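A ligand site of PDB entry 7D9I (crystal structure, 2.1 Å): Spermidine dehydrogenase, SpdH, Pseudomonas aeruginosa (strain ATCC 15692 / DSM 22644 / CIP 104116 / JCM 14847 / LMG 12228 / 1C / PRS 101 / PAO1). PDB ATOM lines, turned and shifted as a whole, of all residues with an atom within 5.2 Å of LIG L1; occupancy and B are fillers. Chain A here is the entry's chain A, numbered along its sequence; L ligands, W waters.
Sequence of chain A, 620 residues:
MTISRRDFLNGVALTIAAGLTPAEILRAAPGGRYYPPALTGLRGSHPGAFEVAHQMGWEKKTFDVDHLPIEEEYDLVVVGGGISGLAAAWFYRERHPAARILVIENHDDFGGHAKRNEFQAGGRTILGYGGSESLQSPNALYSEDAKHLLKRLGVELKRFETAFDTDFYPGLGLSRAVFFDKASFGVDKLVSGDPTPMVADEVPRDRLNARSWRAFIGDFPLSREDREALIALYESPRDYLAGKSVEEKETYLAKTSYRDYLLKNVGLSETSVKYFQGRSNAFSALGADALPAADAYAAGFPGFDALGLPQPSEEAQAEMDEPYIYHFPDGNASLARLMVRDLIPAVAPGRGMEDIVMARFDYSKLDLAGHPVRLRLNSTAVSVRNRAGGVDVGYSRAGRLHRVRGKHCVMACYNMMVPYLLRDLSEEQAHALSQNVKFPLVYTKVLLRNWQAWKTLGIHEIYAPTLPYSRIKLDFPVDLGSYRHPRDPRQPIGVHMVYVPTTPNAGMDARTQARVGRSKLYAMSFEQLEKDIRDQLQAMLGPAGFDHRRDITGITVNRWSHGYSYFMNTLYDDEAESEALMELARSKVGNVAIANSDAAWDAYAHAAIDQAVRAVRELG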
ATOM      1  N   SER A  45     -33.224  34.764  25.846  1.00  0.00           N
ATOM      2  CA  SER A  45     -31.883  35.084  25.389  1.00  0.00           C
ATOM      3  C   SER A  45     -31.992  35.940  24.128  1.00  0.00           C
ATOM      4  O   SER A  45     -31.958  35.445  22.998  1.00  0.00           O
ATOM      5  CB  SER A  45     -31.075  33.807  25.161  1.00  0.00           C
ATOM      6  OG  SER A  45     -30.854  33.153  26.394  1.00  0.00           O
ATOM      7  N   ALA A  49     -27.392  39.463  23.921  1.00  0.00           N
ATOM      8  CA  ALA A  49     -27.030  38.695  25.098  1.00  0.00           C
ATOM      9  C   ALA A  49     -25.969  37.646  24.834  1.00  0.00           C
ATOM     10  O   ALA A  49     -25.255  37.260  25.766  1.00  0.00           O
ATOM     11  CB  ALA A  49     -28.268  38.002  25.681  1.00  0.00           C
ATOM     12  N   PHE A  50     -25.839  37.170  23.601  1.00  0.00           N
ATOM     13  CA  PHE A  50     -25.129  35.932  23.342  1.00  0.00           C
ATOM     14  C   PHE A  50     -23.967  36.085  22.374  1.00  0.00           C
ATOM     15  O   PHE A  50     -23.221  35.118  22.192  1.00  0.00           O
ATOM     16  CB  PHE A  50     -26.108  34.880  22.806  1.00  0.00           C
ATOM     17  CG  PHE A  50     -26.846  35.318  21.556  1.00  0.00           C
ATOM     18  CD1 PHE A  50     -28.083  35.927  21.645  1.00  0.00           C
ATOM     19  CD2 PHE A  50     -26.260  35.159  20.307  1.00  0.00           C
ATOM     20  CE1 PHE A  50     -28.752  36.357  20.495  1.00  0.00           C
ATOM     21  CE2 PHE A  50     -26.925  35.575  19.154  1.00  0.00           C
ATOM     22  CZ  PHE A  50     -28.162  36.176  19.249  1.00  0.00           C
ATOM     23  N   ALA A  53     -20.443  35.545  23.890  1.00  0.00           N
ATOM     24  CA  ALA A  53     -20.408  34.124  24.212  1.00  0.00           C
ATOM     25  C   ALA A  53     -20.162  33.250  22.991  1.00  0.00           C
ATOM     26  O   ALA A  53     -19.363  32.292  23.050  1.00  0.00           O
ATOM     27  CB  ALA A  53     -21.731  33.718  24.884  1.00  0.00           C
ATOM     28  N   HIS A  54     -20.832  33.539  21.865  1.00  0.00           N
ATOM     29  CA  HIS A  54     -20.644  32.720  20.666  1.00  0.00           C
ATOM     30  C   HIS A  54     -19.325  32.999  19.949  1.00  0.00           C
ATOM     31  O   HIS A  54     -18.797  32.107  19.265  1.00  0.00           O
ATOM     32  CB  HIS A  54     -21.791  32.931  19.706  1.00  0.00           C
ATOM     33  CG  HIS A  54     -23.022  32.204  20.106  1.00  0.00           C
ATOM     34  ND1 HIS A  54     -24.246  32.408  19.501  1.00  0.00           N
ATOM     35  CD2 HIS A  54     -23.230  31.271  21.060  1.00  0.00           C
ATOM     36  CE1 HIS A  54     -25.146  31.627  20.061  1.00  0.00           C
ATOM     37  NE2 HIS A  54     -24.550  30.915  20.998  1.00  0.00           N
ATOM     38  N   GLY A  57     -17.493  30.558  21.917  1.00  0.00           N
ATOM     39  CA  GLY A  57     -17.943  29.186  21.754  1.00  0.00           C
ATOM     40  C   GLY A  57     -17.855  28.663  20.330  1.00  0.00           C
ATOM     41  O   GLY A  57     -17.513  27.492  20.122  1.00  0.00           O
ATOM     42  N   TRP A  58     -18.168  29.496  19.335  1.00  0.00           N
ATOM     43  CA  TRP A  58     -18.199  29.053  17.947  1.00  0.00           C
ATOM     44  C   TRP A  58     -16.921  29.393  17.204  1.00  0.00           C
ATOM     45  O   TRP A  58     -16.331  28.527  16.547  1.00  0.00           O
ATOM     46  CB  TRP A  58     -19.371  29.676  17.163  1.00  0.00           C
ATOM     47  CG  TRP A  58     -20.740  29.352  17.674  1.00  0.00           C
ATOM     48  CD1 TRP A  58     -21.053  28.536  18.718  1.00  0.00           C
ATOM     49  CD2 TRP A  58     -21.969  29.831  17.142  1.00  0.00           C
ATOM     50  NE1 TRP A  58     -22.425  28.492  18.886  1.00  0.00           N
ATOM     51  CE2 TRP A  58     -23.012  29.272  17.923  1.00  0.00           C
ATOM     52  CE3 TRP A  58     -22.311  30.692  16.084  1.00  0.00           C
ATOM     53  CZ2 TRP A  58     -24.354  29.545  17.688  1.00  0.00           C
ATOM     54  CZ3 TRP A  58     -23.642  30.960  15.856  1.00  0.00           C
ATOM     55  CH2 TRP A  58     -24.651  30.385  16.645  1.00  0.00           C
ATOM     56  N   LYS A  60     -14.073  30.398  18.559  1.00  0.00           N
ATOM     57  CA  LYS A  60     -12.866  30.169  19.367  1.00  0.00           C
ATOM     58  C   LYS A  60     -12.011  31.432  19.517  1.00  0.00           C
ATOM     59  O   LYS A  60     -10.793  31.359  19.699  1.00  0.00           O
ATOM     60  CB  LYS A  60     -12.034  29.022  18.800  1.00  0.00           C
ATOM     61  CG  LYS A  60     -12.819  27.742  18.573  1.00  0.00           C
ATOM     62  CD  LYS A  60     -13.158  27.089  19.909  1.00  0.00           C
ATOM     63  CE  LYS A  60     -13.476  25.615  19.729  1.00  0.00           C
ATOM     64  NZ  LYS A  60     -14.935  25.389  19.618  1.00  0.00           N
ATOM     65  N   ASN A 106     -24.833  38.568  31.588  1.00  0.00           N
ATOM     66  CA  ASN A 106     -24.797  38.969  30.189  1.00  0.00           C
ATOM     67  C   ASN A 106     -26.156  39.406  29.619  1.00  0.00           C
ATOM     68  O   ASN A 106     -26.183  40.106  28.600  1.00  0.00           O
ATOM     69  CB  ASN A 106     -24.262  37.813  29.340  1.00  0.00           C
ATOM     70  CG  ASN A 106     -25.121  36.582  29.497  1.00  0.00           C
ATOM     71  OD1 ASN A 106     -25.385  36.155  30.610  1.00  0.00           O
ATOM     72  ND2 ASN A 106     -25.628  36.065  28.393  1.00  0.00           N
ATOM     73  N   HIS A 107     -27.285  39.017  30.220  1.00  0.00           N
ATOM     74  CA  HIS A 107     -28.577  39.447  29.699  1.00  0.00           C
ATOM     75  C   HIS A 107     -28.824  40.913  30.096  1.00  0.00           C
ATOM     76  O   HIS A 107     -28.050  41.511  30.846  1.00  0.00           O
ATOM     77  CB  HIS A 107     -29.710  38.569  30.233  1.00  0.00           C
ATOM     78  CG  HIS A 107     -29.798  37.225  29.596  1.00  0.00           C
ATOM     79  ND1 HIS A 107     -29.128  36.128  30.076  1.00  0.00           N
ATOM     80  CD2 HIS A 107     -30.500  36.806  28.517  1.00  0.00           C
ATOM     81  CE1 HIS A 107     -29.403  35.081  29.308  1.00  0.00           C
ATOM     82  NE2 HIS A 107     -30.228  35.463  28.356  1.00  0.00           N
ATOM     83  N   TYR A 414     -23.878  29.095  32.814  1.00  0.00           N
ATOM     84  CA  TYR A 414     -23.993  27.804  32.136  1.00  0.00           C
ATOM     85  C   TYR A 414     -22.677  27.051  32.231  1.00  0.00           C
ATOM     86  O   TYR A 414     -21.617  27.581  31.898  1.00  0.00           O
ATOM     87  CB  TYR A 414     -24.321  28.002  30.651  1.00  0.00           C
ATOM     88  CG  TYR A 414     -25.525  28.836  30.323  1.00  0.00           C
ATOM     89  CD1 TYR A 414     -26.618  28.897  31.181  1.00  0.00           C
ATOM     90  CD2 TYR A 414     -25.599  29.508  29.124  1.00  0.00           C
ATOM     91  CE1 TYR A 414     -27.726  29.637  30.856  1.00  0.00           C
ATOM     92  CE2 TYR A 414     -26.693  30.241  28.783  1.00  0.00           C
ATOM     93  CZ  TYR A 414     -27.746  30.315  29.634  1.00  0.00           C
ATOM     94  OH  TYR A 414     -28.869  31.049  29.284  1.00  0.00           O
ATOM     95  N   MET A 416     -21.424  24.677  30.472  1.00  0.00           N
ATOM     96  CA  MET A 416     -20.760  24.572  29.178  1.00  0.00           C
ATOM     97  C   MET A 416     -19.979  25.831  28.822  1.00  0.00           C
ATOM     98  O   MET A 416     -19.079  25.779  27.983  1.00  0.00           O
ATOM     99  CB  MET A 416     -21.816  24.314  28.108  1.00  0.00           C
ATOM    100  CG  MET A 416     -22.831  25.458  28.269  1.00  0.00           C
ATOM    101  SD  MET A 416     -23.738  26.092  26.930  1.00  0.00           S
ATOM    102  CE  MET A 416     -22.763  27.454  26.378  1.00  0.00           C
ATOM    103  N   MET A 417     -20.336  26.965  29.436  1.00  0.00           N
ATOM    104  CA  MET A 417     -19.591  28.192  29.222  1.00  0.00           C
ATOM    105  C   MET A 417     -18.274  28.218  29.994  1.00  0.00           C
ATOM    106  O   MET A 417     -17.342  28.903  29.575  1.00  0.00           O
ATOM    107  CB  MET A 417     -20.449  29.402  29.598  1.00  0.00           C
ATOM    108  CG  MET A 417     -19.801  30.753  29.411  1.00  0.00           C
ATOM    109  SD  MET A 417     -20.159  31.492  27.804  1.00  0.00           S
ATOM    110  CE  MET A 417     -18.586  31.200  26.969  1.00  0.00           C
ATOM    111  N   TYR A 420     -14.578  28.000  28.492  1.00  0.00           N
ATOM    112  CA  TYR A 420     -14.168  29.150  27.699  1.00  0.00           C
ATOM    113  C   TYR A 420     -13.706  30.302  28.570  1.00  0.00           C
ATOM    114  O   TYR A 420     -13.092  31.241  28.054  1.00  0.00           O
ATOM    115  CB  TYR A 420     -15.314  29.583  26.784  1.00  0.00           C
ATOM    116  CG  TYR A 420     -15.680  28.518  25.768  1.00  0.00           C
ATOM    117  CD1 TYR A 420     -14.930  28.348  24.615  1.00  0.00           C
ATOM    118  CD2 TYR A 420     -16.746  27.647  26.005  1.00  0.00           C
ATOM    119  CE1 TYR A 420     -15.226  27.357  23.697  1.00  0.00           C
ATOM    120  CE2 TYR A 420     -17.061  26.651  25.084  1.00  0.00           C
ATOM    121  CZ  TYR A 420     -16.297  26.516  23.925  1.00  0.00           C
ATOM    122  OH  TYR A 420     -16.566  25.549  23.001  1.00  0.00           O
ATOM    123  N   SER A 434     -18.280  20.519  29.520  1.00  0.00           N
ATOM    124  CA  SER A 434     -18.873  20.588  28.189  1.00  0.00           C
ATOM    125  C   SER A 434     -19.900  19.488  27.958  1.00  0.00           C
ATOM    126  O   SER A 434     -20.731  19.610  27.053  1.00  0.00           O
ATOM    127  CB  SER A 434     -17.767  20.519  27.133  1.00  0.00           C
ATOM    128  OG  SER A 434     -17.494  19.171  26.781  1.00  0.00           O
ATOM    129  N   VAL A 437     -25.013  19.404  28.122  1.00  0.00           N
ATOM    130  CA  VAL A 437     -25.680  20.025  26.989  1.00  0.00           C
ATOM    131  C   VAL A 437     -27.101  20.390  27.425  1.00  0.00           C
ATOM    132  O   VAL A 437     -27.913  19.509  27.722  1.00  0.00           O
ATOM    133  CB  VAL A 437     -25.673  19.107  25.769  1.00  0.00           C
ATOM    134  CG1 VAL A 437     -26.267  19.815  24.568  1.00  0.00           C
ATOM    135  CG2 VAL A 437     -24.216  18.632  25.471  1.00  0.00           C
ATOM    136  N   ARG A 515     -28.803  20.054  20.767  1.00  0.00           N
ATOM    137  CA  ARG A 515     -27.985  20.882  19.873  1.00  0.00           C
ATOM    138  C   ARG A 515     -28.727  21.228  18.593  1.00  0.00           C
ATOM    139  O   ARG A 515     -28.731  22.392  18.147  1.00  0.00           O
ATOM    140  CB  ARG A 515     -26.679  20.157  19.536  1.00  0.00           C
ATOM    141  CG  ARG A 515     -25.688  20.072  20.686  1.00  0.00           C
ATOM    142  CD  ARG A 515     -24.379  19.488  20.178  1.00  0.00           C
ATOM    143  NE  ARG A 515     -23.513  19.059  21.269  1.00  0.00           N
ATOM    144  CZ  ARG A 515     -23.340  17.783  21.618  1.00  0.00           C
ATOM    145  NH1 ARG A 515     -23.989  16.816  20.976  1.00  0.00           N
ATOM    146  NH2 ARG A 515     -22.509  17.477  22.610  1.00  0.00           N
ATOM    147  N   ARG A 518     -31.317  23.863  19.011  1.00  0.00           N
ATOM    148  CA  ARG A 518     -30.767  25.218  19.034  1.00  0.00           C
ATOM    149  C   ARG A 518     -30.465  25.724  17.630  1.00  0.00           C
ATOM    150  O   ARG A 518     -30.628  26.922  17.344  1.00  0.00           O
ATOM    151  CB  ARG A 518     -29.493  25.247  19.875  1.00  0.00           C
ATOM    152  CG  ARG A 518     -29.648  25.673  21.276  1.00  0.00           C
ATOM    153  CD  ARG A 518     -28.258  25.809  21.943  1.00  0.00           C
ATOM    154  NE  ARG A 518     -27.646  24.530  22.285  1.00  0.00           N
ATOM    155  CZ  ARG A 518     -28.058  23.727  23.278  1.00  0.00           C
ATOM    156  NH1 ARG A 518     -29.115  24.064  24.016  1.00  0.00           N
ATOM    157  NH2 ARG A 518     -27.425  22.594  23.526  1.00  0.00           N
ATOM    158  N   SER A 519     -30.008  24.844  16.722  1.00  0.00           N
ATOM    159  CA  SER A 519     -29.767  25.281  15.353  1.00  0.00           C
ATOM    160  C   SER A 519     -31.065  25.701  14.690  1.00  0.00           C
ATOM    161  O   SER A 519     -31.085  26.674  13.920  1.00  0.00           O
ATOM    162  CB  SER A 519     -29.099  24.175  14.516  1.00  0.00           C
ATOM    163  OG  SER A 519     -28.175  23.436  15.268  1.00  0.00           O
ATOM    164  N   LEU A 521     -33.705  26.984  16.235  1.00  0.00           N
ATOM    165  CA  LEU A 521     -34.088  28.279  16.768  1.00  0.00           C
ATOM    166  C   LEU A 521     -33.177  29.379  16.234  1.00  0.00           C
ATOM    167  O   LEU A 521     -33.627  30.503  16.025  1.00  0.00           O
ATOM    168  CB  LEU A 521     -34.035  28.279  18.300  1.00  0.00           C
ATOM    169  CG  LEU A 521     -35.092  27.484  19.075  1.00  0.00           C
ATOM    170  CD1 LEU A 521     -34.834  27.598  20.590  1.00  0.00           C
ATOM    171  CD2 LEU A 521     -36.510  27.946  18.701  1.00  0.00           C
ATOM    172  N   TYR A 522     -31.903  29.057  16.004  1.00  0.00           N
ATOM    173  CA  TYR A 522     -31.004  30.054  15.445  1.00  0.00           C
ATOM    174  C   TYR A 522     -31.409  30.433  14.031  1.00  0.00           C
ATOM    175  O   TYR A 522     -31.135  31.559  13.598  1.00  0.00           O
ATOM    176  CB  TYR A 522     -29.562  29.552  15.474  1.00  0.00           C
ATOM    177  CG  TYR A 522     -28.560  30.648  15.227  1.00  0.00           C
ATOM    178  CD1 TYR A 522     -28.385  31.654  16.158  1.00  0.00           C
ATOM    179  CD2 TYR A 522     -27.798  30.683  14.072  1.00  0.00           C
ATOM    180  CE1 TYR A 522     -27.464  32.676  15.942  1.00  0.00           C
ATOM    181  CE2 TYR A 522     -26.871  31.686  13.846  1.00  0.00           C
ATOM    182  CZ  TYR A 522     -26.705  32.679  14.794  1.00  0.00           C
ATOM    183  OH  TYR A 522     -25.798  33.700  14.599  1.00  0.00           O
ATOM    184  N   ARG A 559     -37.129  33.102  24.356  1.00  0.00           N
ATOM    185  CA  ARG A 559     -36.357  32.082  23.644  1.00  0.00           C
ATOM    186  C   ARG A 559     -35.222  31.608  24.555  1.00  0.00           C
ATOM    187  O   ARG A 559     -34.218  32.297  24.715  1.00  0.00           O
ATOM    188  CB  ARG A 559     -35.810  32.673  22.337  1.00  0.00           C
ATOM    189  CG  ARG A 559     -34.927  31.735  21.525  1.00  0.00           C
ATOM    190  CD  ARG A 559     -34.383  32.426  20.278  1.00  0.00           C
ATOM    191  NE  ARG A 559     -33.598  33.614  20.585  1.00  0.00           N
ATOM    192  CZ  ARG A 559     -33.153  34.459  19.650  1.00  0.00           C
ATOM    193  NH1 ARG A 559     -33.427  34.218  18.365  1.00  0.00           N
ATOM    194  NH2 ARG A 559     -32.427  35.527  19.987  1.00  0.00           N
ATOM    195  N   SER A 561     -32.670  29.345  24.455  1.00  0.00           N
ATOM    196  CA  SER A 561     -31.867  28.459  23.611  1.00  0.00           C
ATOM    197  C   SER A 561     -31.034  27.483  24.443  1.00  0.00           C
ATOM    198  O   SER A 561     -30.886  26.313  24.077  1.00  0.00           O
ATOM    199  CB  SER A 561     -30.998  29.331  22.718  1.00  0.00           C
ATOM    200  OG  SER A 561     -31.819  29.964  21.747  1.00  0.00           O
ATOM    201  N   HIS A 562     -30.508  27.947  25.573  1.00  0.00           N
ATOM    202  CA  HIS A 562     -29.871  27.105  26.578  1.00  0.00           C
ATOM    203  C   HIS A 562     -30.782  27.106  27.821  1.00  0.00           C
ATOM    204  O   HIS A 562     -30.620  27.927  28.729  1.00  0.00           O
ATOM    205  CB  HIS A 562     -28.455  27.594  26.879  1.00  0.00           C
ATOM    206  CG  HIS A 562     -27.527  27.525  25.695  1.00  0.00           C
ATOM    207  ND1 HIS A 562     -26.801  26.394  25.376  1.00  0.00           N
ATOM    208  CD2 HIS A 562     -27.195  28.451  24.760  1.00  0.00           C
ATOM    209  CE1 HIS A 562     -26.077  26.620  24.300  1.00  0.00           C
ATOM    210  NE2 HIS A 562     -26.297  27.862  23.908  1.00  0.00           N
HETATM  211  C1  LIG L   1     -23.541  26.774  21.480  1.00  0.00           C
HETATM  212  C2  LIG L   1     -27.612  28.778  19.650  1.00  0.00           C
HETATM  213  C3  LIG L   1     -27.616  31.933  23.385  1.00  0.00           C
HETATM  214  C4  LIG L   1     -23.292  30.307  24.820  1.00  0.00           C
HETATM  215  C5  LIG L   1     -24.661  27.025  20.685  1.00  0.00           C
HETATM  216  C6  LIG L   1     -25.049  26.278  19.517  1.00  0.00           C
HETATM  217  C7  LIG L   1     -26.145  26.837  19.003  1.00  0.00           C
HETATM  218  C8  LIG L   1     -26.523  27.948  19.843  1.00  0.00           C
HETATM  219  C9  LIG L   1     -26.926  26.351  17.746  1.00  0.00           C
HETATM  220  C10 LIG L   1     -24.288  25.037  18.949  1.00  0.00           C
HETATM  221  C11 LIG L   1     -24.839  23.762  19.580  1.00  0.00           C
HETATM  222  C12 LIG L   1     -24.338  23.582  21.000  1.00  0.00           C
HETATM  223  O1  LIG L   1     -23.087  23.491  21.203  1.00  0.00           O
HETATM  224  O2  LIG L   1     -25.178  23.493  21.943  1.00  0.00           O
HETATM  225  C13 LIG L   1     -27.972  29.819  20.490  1.00  0.00           C
HETATM  226  C14 LIG L   1     -29.094  30.761  20.328  1.00  0.00           C
HETATM  227  C15 LIG L   1     -29.040  31.581  21.384  1.00  0.00           C
HETATM  228  C16 LIG L   1     -27.916  31.248  22.218  1.00  0.00           C
HETATM  229  C17 LIG L   1     -30.156  30.785  19.193  1.00  0.00           C
HETATM  230  C18 LIG L   1     -29.913  32.761  21.773  1.00  0.00           C
HETATM  231  C19 LIG L   1     -30.341  33.594  20.839  1.00  0.00           C
HETATM  232  C20 LIG L   1     -26.481  31.765  24.157  1.00  0.00           C
HETATM  233  C21 LIG L   1     -26.156  32.408  25.419  1.00  0.00           C
HETATM  234  C22 LIG L   1     -24.951  31.925  25.787  1.00  0.00           C
HETATM  235  C23 LIG L   1     -24.488  30.999  24.788  1.00  0.00           C
HETATM  236  C24 LIG L   1     -27.052  33.438  26.171  1.00  0.00           C
HETATM  237  C25 LIG L   1     -24.058  32.242  27.000  1.00  0.00           C
HETATM  238  C26 LIG L   1     -24.007  33.452  27.550  1.00  0.00           C
HETATM  239  C27 LIG L   1     -22.963  29.232  24.027  1.00  0.00           C
HETATM  240  C28 LIG L   1     -21.718  28.530  24.033  1.00  0.00           C
HETATM  241  C29 LIG L   1     -21.776  27.555  23.107  1.00  0.00           C
HETATM  242  C30 LIG L   1     -23.073  27.610  22.474  1.00  0.00           C
HETATM  243  C31 LIG L   1     -20.530  28.855  24.957  1.00  0.00           C
HETATM  244  C32 LIG L   1     -20.679  26.529  22.778  1.00  0.00           C
HETATM  245  C33 LIG L   1     -20.983  25.268  23.600  1.00  0.00           C
HETATM  246  C34 LIG L   1     -19.829  24.290  23.552  1.00  0.00           C
HETATM  247  O3  LIG L   1     -18.931  24.475  22.689  1.00  0.00           O
HETATM  248  O4  LIG L   1     -19.800  23.334  24.364  1.00  0.00           O
HETATM  249  N1  LIG L   1     -25.574  28.037  20.861  1.00  0.00           N
HETATM  250  N2  LIG L   1     -27.285  30.157  21.650  1.00  0.00           N
HETATM  251  N3  LIG L   1     -25.456  30.919  23.806  1.00  0.00           N
HETATM  252  N4  LIG L   1     -23.766  28.651  23.052  1.00  0.00           N
HETATM  253 FE1  LIG L   1     -25.533  29.451  22.387  1.00  0.00          FE
HETATM  254  P1  LG2 L   2     -29.689  30.518  34.932  1.00  0.00           P
HETATM  255  O1  LG2 L   2     -31.003  31.041  35.366  1.00  0.00           O
HETATM  256  O2  LG2 L   2     -29.612  30.055  33.492  1.00  0.00           O
HETATM  257  O3  LG2 L   2     -28.539  31.599  35.273  1.00  0.00           O
HETATM  258  C1  LG2 L   2     -27.230  31.518  34.652  1.00  0.00           C
HETATM  259  C2  LG2 L   2     -26.955  32.859  34.015  1.00  0.00           C
HETATM  260  O4  LG2 L   2     -25.540  33.000  33.691  1.00  0.00           O
HETATM  261  C3  LG2 L   2     -27.731  33.103  32.714  1.00  0.00           C
HETATM  262  O5  LG2 L   2     -28.416  34.354  32.729  1.00  0.00           O
HETATM  263  C4  LG2 L   2     -26.631  33.110  31.646  1.00  0.00           C
HETATM  264  O6  LG2 L   2     -26.937  33.971  30.563  1.00  0.00           O
HETATM  265  C5  LG2 L   2     -25.489  33.693  32.459  1.00  0.00           C
HETATM  266  N1  LG2 L   2     -24.177  33.573  31.814  1.00  0.00           N
HETATM  267  C6  LG2 L   2     -23.774  32.585  30.955  1.00  0.00           C
HETATM  268  N2  LG2 L   2     -22.560  32.754  30.479  1.00  0.00           N
HETATM  269  C7  LG2 L   2     -22.155  33.954  31.049  1.00  0.00           C
HETATM  270  C8  LG2 L   2     -20.966  34.706  30.936  1.00  0.00           C
HETATM  271  N3  LG2 L   2     -19.922  34.347  30.184  1.00  0.00           N
HETATM  272  N4  LG2 L   2     -20.881  35.858  31.629  1.00  0.00           N
HETATM  273  C9  LG2 L   2     -21.929  36.242  32.364  1.00  0.00           C
HETATM  274  N5  LG2 L   2     -23.098  35.614  32.553  1.00  0.00           N
HETATM  275  C10 LG2 L   2     -23.144  34.472  31.866  1.00  0.00           C
HETATM  276  N6  LG2 L   2     -37.220  25.269  37.754  1.00  0.00           N
HETATM  277  C11 LG2 L   2     -38.140  25.078  38.760  1.00  0.00           C
HETATM  278  O7  LG2 L   2     -37.790  24.727  39.896  1.00  0.00           O
HETATM  279  N7  LG2 L   2     -39.477  25.270  38.491  1.00  0.00           N
HETATM  280  C12 LG2 L   2     -40.023  25.664  37.279  1.00  0.00           C
HETATM  281  O8  LG2 L   2     -41.228  25.808  37.166  1.00  0.00           O
HETATM  282  C13 LG2 L   2     -39.037  25.869  36.225  1.00  0.00           C
HETATM  283  N8  LG2 L   2     -39.462  26.235  35.019  1.00  0.00           N
HETATM  284  C14 LG2 L   2     -38.500  26.448  34.037  1.00  0.00           C
HETATM  285  C15 LG2 L   2     -38.905  26.865  32.758  1.00  0.00           C
HETATM  286  C16 LG2 L   2     -37.966  27.073  31.736  1.00  0.00           C
HETATM  287  C17 LG2 L   2     -38.418  27.525  30.372  1.00  0.00           C
HETATM  288  C18 LG2 L   2     -36.606  26.872  32.004  1.00  0.00           C
HETATM  289  C19 LG2 L   2     -35.563  27.110  30.935  1.00  0.00           C
HETATM  290  C20 LG2 L   2     -36.203  26.471  33.273  1.00  0.00           C
HETATM  291  C21 LG2 L   2     -37.127  26.256  34.280  1.00  0.00           C
HETATM  292  N9  LG2 L   2     -36.731  25.862  35.579  1.00  0.00           N
HETATM  293  C22 LG2 L   2     -37.655  25.659  36.567  1.00  0.00           C
HETATM  294  C23 LG2 L   2     -35.316  25.585  35.887  1.00  0.00           C
HETATM  295  C24 LG2 L   2     -34.429  26.817  35.944  1.00  0.00           C
HETATM  296  O9  LG2 L   2     -33.269  26.578  35.131  1.00  0.00           O
HETATM  297  C25 LG2 L   2     -34.054  27.088  37.400  1.00  0.00           C
HETATM  298  O10 LG2 L   2     -35.282  27.249  38.107  1.00  0.00           O
HETATM  299  C26 LG2 L   2     -33.242  28.370  37.586  1.00  0.00           C
HETATM  300  O11 LG2 L   2     -33.976  29.468  37.049  1.00  0.00           O
HETATM  301  C27 LG2 L   2     -31.857  28.270  36.975  1.00  0.00           C
HETATM  302  O12 LG2 L   2     -30.969  29.156  37.681  1.00  0.00           O
HETATM  303  P2  LG2 L   2     -29.422  29.141  37.422  1.00  0.00           P
HETATM  304  O13 LG2 L   2     -28.917  27.741  37.769  1.00  0.00           O
HETATM  305  O14 LG2 L   2     -28.848  30.376  38.120  1.00  0.00           O
HETATM  306  O15 LG2 L   2     -29.273  29.282  35.842  1.00  0.00           O
HETATM  307  O   HOH W   1     -22.230  21.111  22.404  1.00  0.00           O
HETATM  308  O   HOH W   2     -21.854  21.744  25.422  1.00  0.00           O
HETATM  309  O   HOH W   3     -18.147  23.680  26.694  1.00  0.00           O
HETATM  310  O   HOH W   4     -24.236  23.008  24.512  1.00  0.00           O
HETATM  311  O   HOH W   5     -18.365  20.809  23.384  1.00  0.00           O
HETATM  312  O   HOH W   6     -18.537  25.009  20.095  1.00  0.00           O
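Water W6 lies within hydrogen-bond range of an oxygen (O3) of LIG L1 (2.7 Å) and the backbone carbonyl oxygen of Gly 57 (2.7 Å). Water W4 bridges O2 of LIG L1 and NH2 of Arg 518. Water W1 lies within hydrogen-bond range of NE of Arg 515 and O1 of LIG L1. Water W2 bridges O4 of LIG L1 (2.8 Å) and O of Ser 434 (2.9 Å). Water W3 lies within hydrogen-bond range of O of Met 416 (2.6 Å) and O4 of LIG L1 (2.9 Å).
NE2 of His 54 binds FE1 of LIG L1, 2.2 Å away. NE2 of His 562 binds FE1 of LIG L1, at 2.3 Å. The side-chain hydroxyl (OH) of Tyr 420 is in hydrogen-bond range of an oxygen (O3) of LIG L1, at 2.6 Å. O2 of LIG L1 lies within salt-bridge range of NE of Arg 518 (2.7 Å). OD1 of Asn 106 sits at hydrogen-bond distance from O6 of LG2 L2. N3 of LG2 L2 lies close to SD of Met 417 (3.7 Å). A ring nitrogen (ND1) of His 107 lies close to an oxygen (O6) of LG2 L2, at 3.1 Å.
O of Ser 45 touches C19 of LIG L1, 3.3 Å away. Phe 50 touches LIG L1 (CE1 to C19, 3.2 Å). Ala 53 touches LIG L1. Gly 57 touches LIG L1 (CA to C32, 3.9 Å). NE1 of Trp 58 touches C5 of LIG L1, at 3.2 Å. Asn 106 touches LIG L1 (ND2 to C26, 3.2 Å). CE2 of Tyr 414 touches C25 of LIG L1, at 3.8 Å. Met 416 touches LIG L1 (CE to C28, 2.8 Å). Met 417 touches LIG L1. CG of Arg 515 touches O2 of LIG L1 (3.7 Å). N of Ser 519 touches C9 of LIG L1 (3.6 Å). CD1 of Tyr 522 touches C17 of LIG L1, at 3.6 Å. NH2 of Arg 559 touches C19 of LIG L1, at 3.0 Å. Ser 561 touches LIG L1 (OG to C17, 3.2 Å). Of the 24 residues printed, 18 come within 4 Å of LIG L1. The nearest printed residue that does not touch LIG L1 is Ala 49 (4.2 Å).
ND1 of His 562 lies within hydrogen-bond range of SD of Met 416 (3.4 Å). O of Ser 561 lies within hydrogen-bond range of NH1 of Arg 518, at 2.9 Å. The backbone carbonyl oxygen (O) of Arg 559 lies within hydrogen-bond range of the backbone NH (N) of Ser 45 (2.9 Å). ND2 of Asn 106 is in hydrogen-bond range of O of Ala 49, at 2.9 Å. NE2 of His 107 lies within hydrogen-bond range of OG of Ser 45, 3.1 Å away. The side-chain hydroxyl (OG) of Ser 519 is in hydrogen-bond range of the backbone carbonyl oxygen (O) of Arg 515 (3.1 Å). O of Gly 57 lies within hydrogen-bond range of NZ of Lys 60, 3.4 Å away.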
